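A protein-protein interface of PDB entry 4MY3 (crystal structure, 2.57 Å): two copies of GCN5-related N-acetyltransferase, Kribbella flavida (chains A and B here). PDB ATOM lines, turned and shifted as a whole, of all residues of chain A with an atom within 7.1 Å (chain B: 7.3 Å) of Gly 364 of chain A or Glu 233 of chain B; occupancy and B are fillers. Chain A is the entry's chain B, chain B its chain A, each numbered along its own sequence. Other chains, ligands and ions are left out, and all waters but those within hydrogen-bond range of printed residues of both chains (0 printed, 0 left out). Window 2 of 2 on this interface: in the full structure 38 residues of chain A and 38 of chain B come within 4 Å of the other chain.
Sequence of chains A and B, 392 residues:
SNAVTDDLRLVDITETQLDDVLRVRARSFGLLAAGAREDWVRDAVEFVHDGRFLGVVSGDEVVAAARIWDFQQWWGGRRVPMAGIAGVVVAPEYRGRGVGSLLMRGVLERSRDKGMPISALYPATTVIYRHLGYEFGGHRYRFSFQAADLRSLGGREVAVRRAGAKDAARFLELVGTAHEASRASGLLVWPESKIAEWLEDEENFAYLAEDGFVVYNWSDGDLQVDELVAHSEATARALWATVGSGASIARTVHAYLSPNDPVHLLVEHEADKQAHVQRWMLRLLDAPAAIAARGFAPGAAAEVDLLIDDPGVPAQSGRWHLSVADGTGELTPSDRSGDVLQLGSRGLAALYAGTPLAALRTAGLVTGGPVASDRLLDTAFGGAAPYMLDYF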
ATOM      1  N   ARG A 346      19.289  28.011 -38.818  1.00  0.00           N
ATOM      2  CA  ARG A 346      20.414  28.405 -37.982  1.00  0.00           C
ATOM      3  C   ARG A 346      21.555  27.388 -38.074  1.00  0.00           C
ATOM      4  O   ARG A 346      22.717  27.762 -38.225  1.00  0.00           O
ATOM      5  CB  ARG A 346      19.959  28.591 -36.531  1.00  0.00           C
ATOM      6  CG  ARG A 346      19.026  29.784 -36.301  1.00  0.00           C
ATOM      7  CD  ARG A 346      18.463  29.797 -34.887  1.00  0.00           C
ATOM      8  NE  ARG A 346      19.505  29.835 -33.860  1.00  0.00           N
ATOM      9  CZ  ARG A 346      19.299  29.496 -32.587  1.00  0.00           C
ATOM     10  NH1 ARG A 346      20.280  29.560 -31.697  1.00  0.00           N
ATOM     11  NH2 ARG A 346      18.093  29.094 -32.202  1.00  0.00           N
ATOM     12  N   ALA A 358      29.799  18.799 -33.660  1.00  0.00           N
ATOM     13  CA  ALA A 358      29.650  18.534 -32.223  1.00  0.00           C
ATOM     14  C   ALA A 358      28.977  19.701 -31.501  1.00  0.00           C
ATOM     15  O   ALA A 358      28.067  19.498 -30.688  1.00  0.00           O
ATOM     16  CB  ALA A 358      30.995  18.246 -31.591  1.00  0.00           C
ATOM     17  N   ALA A 359      29.423  20.917 -31.814  1.00  0.00           N
ATOM     18  CA  ALA A 359      28.869  22.126 -31.217  1.00  0.00           C
ATOM     19  C   ALA A 359      27.391  22.320 -31.558  1.00  0.00           C
ATOM     20  O   ALA A 359      26.576  22.589 -30.675  1.00  0.00           O
ATOM     21  CB  ALA A 359      29.659  23.323 -31.670  1.00  0.00           C
ATOM     22  N   LEU A 360      27.055  22.189 -32.841  1.00  0.00           N
ATOM     23  CA  LEU A 360      25.680  22.376 -33.295  1.00  0.00           C
ATOM     24  C   LEU A 360      24.749  21.339 -32.708  1.00  0.00           C
ATOM     25  O   LEU A 360      23.608  21.650 -32.378  1.00  0.00           O
ATOM     26  CB  LEU A 360      25.593  22.340 -34.813  1.00  0.00           C
ATOM     27  CG  LEU A 360      26.429  23.424 -35.476  1.00  0.00           C
ATOM     28  CD1 LEU A 360      26.358  23.294 -36.982  1.00  0.00           C
ATOM     29  CD2 LEU A 360      25.980  24.806 -35.013  1.00  0.00           C
ATOM     30  N   ARG A 361      25.231  20.108 -32.587  1.00  0.00           N
ATOM     31  CA  ARG A 361      24.448  19.055 -31.960  1.00  0.00           C
ATOM     32  C   ARG A 361      24.161  19.382 -30.498  1.00  0.00           C
ATOM     33  O   ARG A 361      23.016  19.280 -30.043  1.00  0.00           O
ATOM     34  CB  ARG A 361      25.161  17.714 -32.059  1.00  0.00           C
ATOM     35  CG  ARG A 361      25.046  17.048 -33.410  1.00  0.00           C
ATOM     36  CD  ARG A 361      25.458  15.593 -33.316  1.00  0.00           C
ATOM     37  NE  ARG A 361      25.524  14.975 -34.635  1.00  0.00           N
ATOM     38  CZ  ARG A 361      24.456  14.617 -35.337  1.00  0.00           C
ATOM     39  NH1 ARG A 361      24.599  14.073 -36.535  1.00  0.00           N
ATOM     40  NH2 ARG A 361      23.245  14.823 -34.844  1.00  0.00           N
ATOM     41  N   THR A 362      25.194  19.787 -29.763  1.00  0.00           N
ATOM     42  CA  THR A 362      25.001  20.154 -28.371  1.00  0.00           C
ATOM     43  C   THR A 362      24.088  21.360 -28.244  1.00  0.00           C
ATOM     44  O   THR A 362      23.259  21.420 -27.348  1.00  0.00           O
ATOM     45  CB  THR A 362      26.312  20.452 -27.690  1.00  0.00           C
ATOM     46  OG1 THR A 362      27.123  19.281 -27.735  1.00  0.00           O
ATOM     47  CG2 THR A 362      26.079  20.832 -26.234  1.00  0.00           C
ATOM     48  N   ALA A 363      24.224  22.324 -29.146  1.00  0.00           N
ATOM     49  CA  ALA A 363      23.341  23.492 -29.125  1.00  0.00           C
ATOM     50  C   ALA A 363      21.924  23.122 -29.592  1.00  0.00           C
ATOM     51  O   ALA A 363      21.015  23.952 -29.582  1.00  0.00           O
ATOM     52  CB  ALA A 363      23.917  24.602 -29.976  1.00  0.00           C
ATOM     53  N   GLY A 364      21.746  21.871 -30.017  1.00  0.00           N
ATOM     54  CA  GLY A 364      20.448  21.395 -30.469  1.00  0.00           C
ATOM     55  C   GLY A 364      20.018  22.043 -31.762  1.00  0.00           C
ATOM     56  O   GLY A 364      18.839  22.139 -32.059  1.00  0.00           O
ATOM     57  N   LEU A 365      21.000  22.466 -32.542  1.00  0.00           N
ATOM     58  CA  LEU A 365      20.772  23.300 -33.715  1.00  0.00           C
ATOM     59  C   LEU A 365      20.673  22.439 -34.969  1.00  0.00           C
ATOM     60  O   LEU A 365      20.236  22.907 -36.017  1.00  0.00           O
ATOM     61  CB  LEU A 365      21.897  24.344 -33.830  1.00  0.00           C
ATOM     62  CG  LEU A 365      21.503  25.838 -33.807  1.00  0.00           C
ATOM     63  CD1 LEU A 365      20.308  26.109 -32.900  1.00  0.00           C
ATOM     64  CD2 LEU A 365      22.679  26.752 -33.460  1.00  0.00           C
ATOM     65  N   VAL A 366      21.107  21.181 -34.844  1.00  0.00           N
ATOM     66  CA  VAL A 366      20.886  20.141 -35.853  1.00  0.00           C
ATOM     67  C   VAL A 366      20.588  18.837 -35.116  1.00  0.00           C
ATOM     68  O   VAL A 366      20.786  18.732 -33.908  1.00  0.00           O
ATOM     69  CB  VAL A 366      22.105  19.934 -36.772  1.00  0.00           C
ATOM     70  CG1 VAL A 366      22.597  21.249 -37.299  1.00  0.00           C
ATOM     71  CG2 VAL A 366      23.212  19.255 -36.027  1.00  0.00           C
ATOM     72  N   THR A 367      20.125  17.828 -35.830  1.00  0.00           N
ATOM     73  CA  THR A 367      19.657  16.634 -35.156  1.00  0.00           C
ATOM     74  C   THR A 367      19.598  15.496 -36.149  1.00  0.00           C
ATOM     75  O   THR A 367      19.562  15.730 -37.351  1.00  0.00           O
ATOM     76  CB  THR A 367      18.250  16.857 -34.555  1.00  0.00           C
ATOM     77  OG1 THR A 367      17.933  15.791 -33.652  1.00  0.00           O
ATOM     78  CG2 THR A 367      17.198  16.910 -35.640  1.00  0.00           C
ATOM     79  N   LEU B 153      18.876  29.873 -18.917  1.00  0.00           N
ATOM     80  CA  LEU B 153      19.112  28.869 -19.936  1.00  0.00           C
ATOM     81  C   LEU B 153      18.202  27.647 -19.761  1.00  0.00           C
ATOM     82  O   LEU B 153      18.005  26.882 -20.691  1.00  0.00           O
ATOM     83  CB  LEU B 153      20.591  28.468 -19.961  1.00  0.00           C
ATOM     84  CG  LEU B 153      21.436  28.959 -21.136  1.00  0.00           C
ATOM     85  CD1 LEU B 153      21.261  28.019 -22.302  1.00  0.00           C
ATOM     86  CD2 LEU B 153      21.012  30.321 -21.560  1.00  0.00           C
ATOM     87  N   GLY B 154      17.630  27.464 -18.584  1.00  0.00           N
ATOM     88  CA  GLY B 154      16.703  26.359 -18.390  1.00  0.00           C
ATOM     89  C   GLY B 154      17.329  25.053 -17.918  1.00  0.00           C
ATOM     90  O   GLY B 154      18.165  25.047 -17.012  1.00  0.00           O
ATOM     91  N   GLY B 155      16.907  23.942 -18.521  1.00  0.00           N
ATOM     92  CA  GLY B 155      17.371  22.618 -18.137  1.00  0.00           C
ATOM     93  C   GLY B 155      17.187  22.209 -16.676  1.00  0.00           C
ATOM     94  O   GLY B 155      17.922  21.361 -16.174  1.00  0.00           O
ATOM     95  N   VAL B 158      17.148  18.550 -15.392  1.00  0.00           N
ATOM     96  CA  VAL B 158      18.381  17.770 -15.402  1.00  0.00           C
ATOM     97  C   VAL B 158      19.039  17.643 -14.027  1.00  0.00           C
ATOM     98  O   VAL B 158      19.257  18.644 -13.346  1.00  0.00           O
ATOM     99  CB  VAL B 158      19.390  18.382 -16.391  1.00  0.00           C
ATOM    100  CG1 VAL B 158      20.723  17.622 -16.369  1.00  0.00           C
ATOM    101  CG2 VAL B 158      18.796  18.399 -17.785  1.00  0.00           C
ATOM    102  N   ASP B 211      26.058  13.230 -18.158  1.00  0.00           N
ATOM    103  CA  ASP B 211      26.909  13.347 -19.337  1.00  0.00           C
ATOM    104  C   ASP B 211      27.589  14.705 -19.430  1.00  0.00           C
ATOM    105  O   ASP B 211      27.637  15.315 -20.503  1.00  0.00           O
ATOM    106  CB  ASP B 211      26.110  13.091 -20.606  1.00  0.00           C
ATOM    107  CG  ASP B 211      25.003  14.094 -20.800  1.00  0.00           C
ATOM    108  OD1 ASP B 211      24.294  14.003 -21.816  1.00  0.00           O
ATOM    109  OD2 ASP B 211      24.831  14.980 -19.938  1.00  0.00           O
ATOM    110  N   ALA B 230      29.749  19.113 -21.539  1.00  0.00           N
ATOM    111  CA  ALA B 230      28.343  18.752 -21.650  1.00  0.00           C
ATOM    112  C   ALA B 230      28.062  18.178 -23.023  1.00  0.00           C
ATOM    113  O   ALA B 230      28.360  18.800 -24.038  1.00  0.00           O
ATOM    114  CB  ALA B 230      27.471  19.960 -21.409  1.00  0.00           C
ATOM    115  N   HIS B 231      27.468  16.994 -23.055  1.00  0.00           N
ATOM    116  CA  HIS B 231      27.253  16.296 -24.314  1.00  0.00           C
ATOM    117  C   HIS B 231      25.894  16.625 -24.935  1.00  0.00           C
ATOM    118  O   HIS B 231      25.808  16.873 -26.137  1.00  0.00           O
ATOM    119  CB  HIS B 231      27.453  14.794 -24.116  1.00  0.00           C
ATOM    120  CG  HIS B 231      28.840  14.434 -23.676  1.00  0.00           C
ATOM    121  ND1 HIS B 231      29.122  13.308 -22.932  1.00  0.00           N
ATOM    122  CD2 HIS B 231      30.026  15.064 -23.871  1.00  0.00           C
ATOM    123  CE1 HIS B 231      30.422  13.258 -22.691  1.00  0.00           C
ATOM    124  NE2 HIS B 231      30.993  14.313 -23.248  1.00  0.00           N
ATOM    125  N   SER B 232      24.848  16.655 -24.115  1.00  0.00           N
ATOM    126  CA  SER B 232      23.519  17.039 -24.585  1.00  0.00           C
ATOM    127  C   SER B 232      23.205  18.516 -24.312  1.00  0.00           C
ATOM    128  O   SER B 232      23.843  19.169 -23.483  1.00  0.00           O
ATOM    129  CB  SER B 232      22.455  16.180 -23.918  1.00  0.00           C
ATOM    130  OG  SER B 232      22.344  16.540 -22.556  1.00  0.00           O
ATOM    131  N   GLU B 233      22.199  19.021 -25.013  1.00  0.00           N
ATOM    132  CA  GLU B 233      21.750  20.405 -24.878  1.00  0.00           C
ATOM    133  C   GLU B 233      21.121  20.695 -23.506  1.00  0.00           C
ATOM    134  O   GLU B 233      21.307  21.771 -22.934  1.00  0.00           O
ATOM    135  CB  GLU B 233      20.737  20.720 -25.988  1.00  0.00           C
ATOM    136  CG  GLU B 233      20.227  22.135 -26.026  1.00  0.00           C
ATOM    137  CD  GLU B 233      18.967  22.253 -26.864  1.00  0.00           C
ATOM    138  OE1 GLU B 233      18.345  23.335 -26.839  1.00  0.00           O
ATOM    139  OE2 GLU B 233      18.587  21.264 -27.542  1.00  0.00           O
ATOM    140  N   ALA B 234      20.373  19.735 -22.987  1.00  0.00           N
ATOM    141  CA  ALA B 234      19.728  19.921 -21.696  1.00  0.00           C
ATOM    142  C   ALA B 234      20.773  19.982 -20.588  1.00  0.00           C
ATOM    143  O   ALA B 234      20.621  20.730 -19.625  1.00  0.00           O
ATOM    144  CB  ALA B 234      18.702  18.805 -21.430  1.00  0.00           C
ATOM    145  N   THR B 235      21.838  19.204 -20.730  1.00  0.00           N
ATOM    146  CA  THR B 235      22.890  19.231 -19.733  1.00  0.00           C
ATOM    147  C   THR B 235      23.658  20.540 -19.818  1.00  0.00           C
ATOM    148  O   THR B 235      23.982  21.143 -18.799  1.00  0.00           O
ATOM    149  CB  THR B 235      23.848  18.033 -19.869  1.00  0.00           C
ATOM    150  OG1 THR B 235      23.149  16.825 -19.540  1.00  0.00           O
ATOM    151  CG2 THR B 235      25.028  18.174 -18.926  1.00  0.00           C
ATOM    152  N   ALA B 236      23.928  21.001 -21.032  1.00  0.00           N
ATOM    153  CA  ALA B 236      24.673  22.245 -21.197  1.00  0.00           C
ATOM    154  C   ALA B 236      23.878  23.364 -20.554  1.00  0.00           C
ATOM    155  O   ALA B 236      24.429  24.252 -19.894  1.00  0.00           O
ATOM    156  CB  ALA B 236      24.935  22.527 -22.665  1.00  0.00           C
ATOM    157  N   ARG B 237      22.564  23.288 -20.718  1.00  0.00           N
ATOM    158  CA  ARG B 237      21.662  24.258 -20.129  1.00  0.00           C
ATOM    159  C   ARG B 237      21.686  24.239 -18.597  1.00  0.00           C
ATOM    160  O   ARG B 237      21.956  25.261 -17.965  1.00  0.00           O
ATOM    161  CB  ARG B 237      20.253  24.049 -20.674  1.00  0.00           C
ATOM    162  CG  ARG B 237      20.109  24.547 -22.102  1.00  0.00           C
ATOM    163  CD  ARG B 237      18.654  24.626 -22.548  1.00  0.00           C
ATOM    164  NE  ARG B 237      18.424  25.914 -23.207  1.00  0.00           N
ATOM    165  CZ  ARG B 237      18.389  26.071 -24.525  1.00  0.00           C
ATOM    166  NH1 ARG B 237      18.543  25.019 -25.311  1.00  0.00           N
ATOM    167  NH2 ARG B 237      18.198  27.267 -25.055  1.00  0.00           N
ATOM    168  N   ALA B 238      21.419  23.086 -17.997  1.00  0.00           N
ATOM    169  CA  ALA B 238      21.443  22.966 -16.540  1.00  0.00           C
ATOM    170  C   ALA B 238      22.783  23.379 -15.898  1.00  0.00           C
ATOM    171  O   ALA B 238      22.808  24.013 -14.834  1.00  0.00           O
ATOM    172  CB  ALA B 238      21.090  21.559 -16.133  1.00  0.00           C
ATOM    173  N   LEU B 239      23.897  23.008 -16.522  1.00  0.00           N
ATOM    174  CA  LEU B 239      25.185  23.333 -15.928  1.00  0.00           C
ATOM    175  C   LEU B 239      25.419  24.857 -15.905  1.00  0.00           C
ATOM    176  O   LEU B 239      25.787  25.414 -14.867  1.00  0.00           O
ATOM    177  CB  LEU B 239      26.329  22.571 -16.610  1.00  0.00           C
ATOM    178  CG  LEU B 239      26.300  21.032 -16.483  1.00  0.00           C
ATOM    179  CD1 LEU B 239      27.463  20.390 -17.234  1.00  0.00           C
ATOM    180  CD2 LEU B 239      26.293  20.575 -15.035  1.00  0.00           C
ATOM    181  N   PRO B 262      29.770  25.692 -27.430  1.00  0.00           N
ATOM    182  CA  PRO B 262      28.340  25.892 -27.697  1.00  0.00           C
ATOM    183  C   PRO B 262      27.595  26.941 -26.849  1.00  0.00           C
ATOM    184  O   PRO B 262      26.452  27.195 -27.184  1.00  0.00           O
ATOM    185  CB  PRO B 262      27.738  24.492 -27.500  1.00  0.00           C
ATOM    186  CG  PRO B 262      28.777  23.711 -26.769  1.00  0.00           C
ATOM    187  CD  PRO B 262      30.099  24.289 -27.145  1.00  0.00           C
ATOM    188  N   LEU B 265      26.069  29.859 -28.815  1.00  0.00           N
ATOM    189  CA  LEU B 265      24.910  29.587 -29.638  1.00  0.00           C
ATOM    190  C   LEU B 265      23.652  29.521 -28.773  1.00  0.00           C
ATOM    191  O   LEU B 265      22.539  29.650 -29.275  1.00  0.00           O
ATOM    192  CB  LEU B 265      25.105  28.289 -30.431  1.00  0.00           C
ATOM    193  CG  LEU B 265      26.321  28.194 -31.357  1.00  0.00           C
ATOM    194  CD1 LEU B 265      26.508  26.772 -31.782  1.00  0.00           C
ATOM    195  CD2 LEU B 265      26.173  29.057 -32.586  1.00  0.00           C
ATOM    196  N   LEU B 266      23.834  29.333 -27.469  1.00  0.00           N
ATOM    197  CA  LEU B 266      22.704  29.142 -26.568  1.00  0.00           C
ATOM    198  C   LEU B 266      22.277  30.416 -25.854  1.00  0.00           C
ATOM    199  O   LEU B 266      21.089  30.678 -25.690  1.00  0.00           O
ATOM    200  CB  LEU B 266      23.032  28.068 -25.525  1.00  0.00           C
ATOM    201  CG  LEU B 266      23.162  26.621 -26.019  1.00  0.00           C
ATOM    202  CD1 LEU B 266      23.804  25.761 -24.952  1.00  0.00           C
ATOM    203  CD2 LEU B 266      21.813  26.066 -26.414  1.00  0.00           C
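O of His 231 of chain B is in hydrogen-bond range of OG1 of Thr 362 of chain A, at 3.2 Å.
NH1 of Arg 346 of chain A sits at hydrogen-bond distance from O of Leu 265 of chain B, at 3.3 Å.
Of the 18 printed residues of chain B, 7 touch a printed residue of chain A.
Printed residues of chain B that touch a printed residue of chain A: Ala 230, His 231, Ser 232, Glu 233, Pro 262, Leu 265 and Leu 266.
Hydrophobic or aromatic side chains of chain B that line the printed part of chain A: Pro 262, Leu 265 and Leu 266.
Of the 11 printed residues of chain A, 6 touch a printed residue of chain B.
Hydrophobic or aromatic side chains of chain A that line the printed part of chain B: Leu 360 and Ala 363.
Along chain A the printed residues that touch a printed residue of chain B span positions 346 to 364.
Among the printed residues, no Asp or Glu carboxylate lies within 4 Å of a Lys or Arg side-chain nitrogen of the other chain.
Ala 359 of chain A touches Pro 262 of chain B (O to CB, 3.9 Å).
Leu 265 of chain B touches Leu 360 of chain A.
Thr 362 of chain A touches Ala 230 of chain B (CG2 to O, 3.8 Å).
Thr 362 of chain A touches Ser 232 of chain B (CG2 to O, 3.9 Å).
Thr 362 of chain A touches Glu 233 of chain B.
CG2 of Thr 362 of chain A touches CG of Pro 262 of chain B (3.98 Å).
O of Ala 363 of chain A touches CD of Glu 233 of chain B (3.8 Å).
Ala 363 of chain A touches Leu 265 of chain B.
Leu 266 of chain B touches Ala 363 of chain A (CD2 to O, 3.9 Å).
Glu 233 of chain B touches Gly 364 of chain A (OE2 to CA, 3.5 Å).
O of Ala 358 of chain A sits at hydrogen-bond distance from OG1 of Thr 362 of chain A (3.1 Å).
O of Asp 211 of chain B is in hydrogen-bond range of N of His 231 of chain B (3.1 Å).
OG1 of Thr 235 of chain B sits at hydrogen-bond distance from OG of Ser 232 of chain B (3.1 Å).
The backbone carbonyl oxygen (O) of Leu 360 of chain A is in hydrogen-bond range of the backbone NH (N) of Leu 365 of chain A (2.7 Å).
OG of Ser 232 of chain B sits at hydrogen-bond distance from OD1 of Asp 211 of chain B, at 3.3 Å.
No position is printed for both chains.
Of chain B, only Glu 233 (3.5 Å) comes within 4 Å of Gly 364 of chain A.
Of the printed residues of chain A, Ser 232 of chain B touches Thr 362.
Of chain A, only Thr 362, Ala 363 and Gly 364 come within 4 Å of Glu 233 of chain B.
Of the printed residues of chain A, Leu 266 of chain B touches Ala 363.
The nearest residue of chain B that does not touch Gly 364 of chain A is Leu 266 of chain B (5.5 Å).
The nearest printed residue of chain A that does not touch Pro 262 of chain B is Ala 363 of chain A (4.4 Å).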
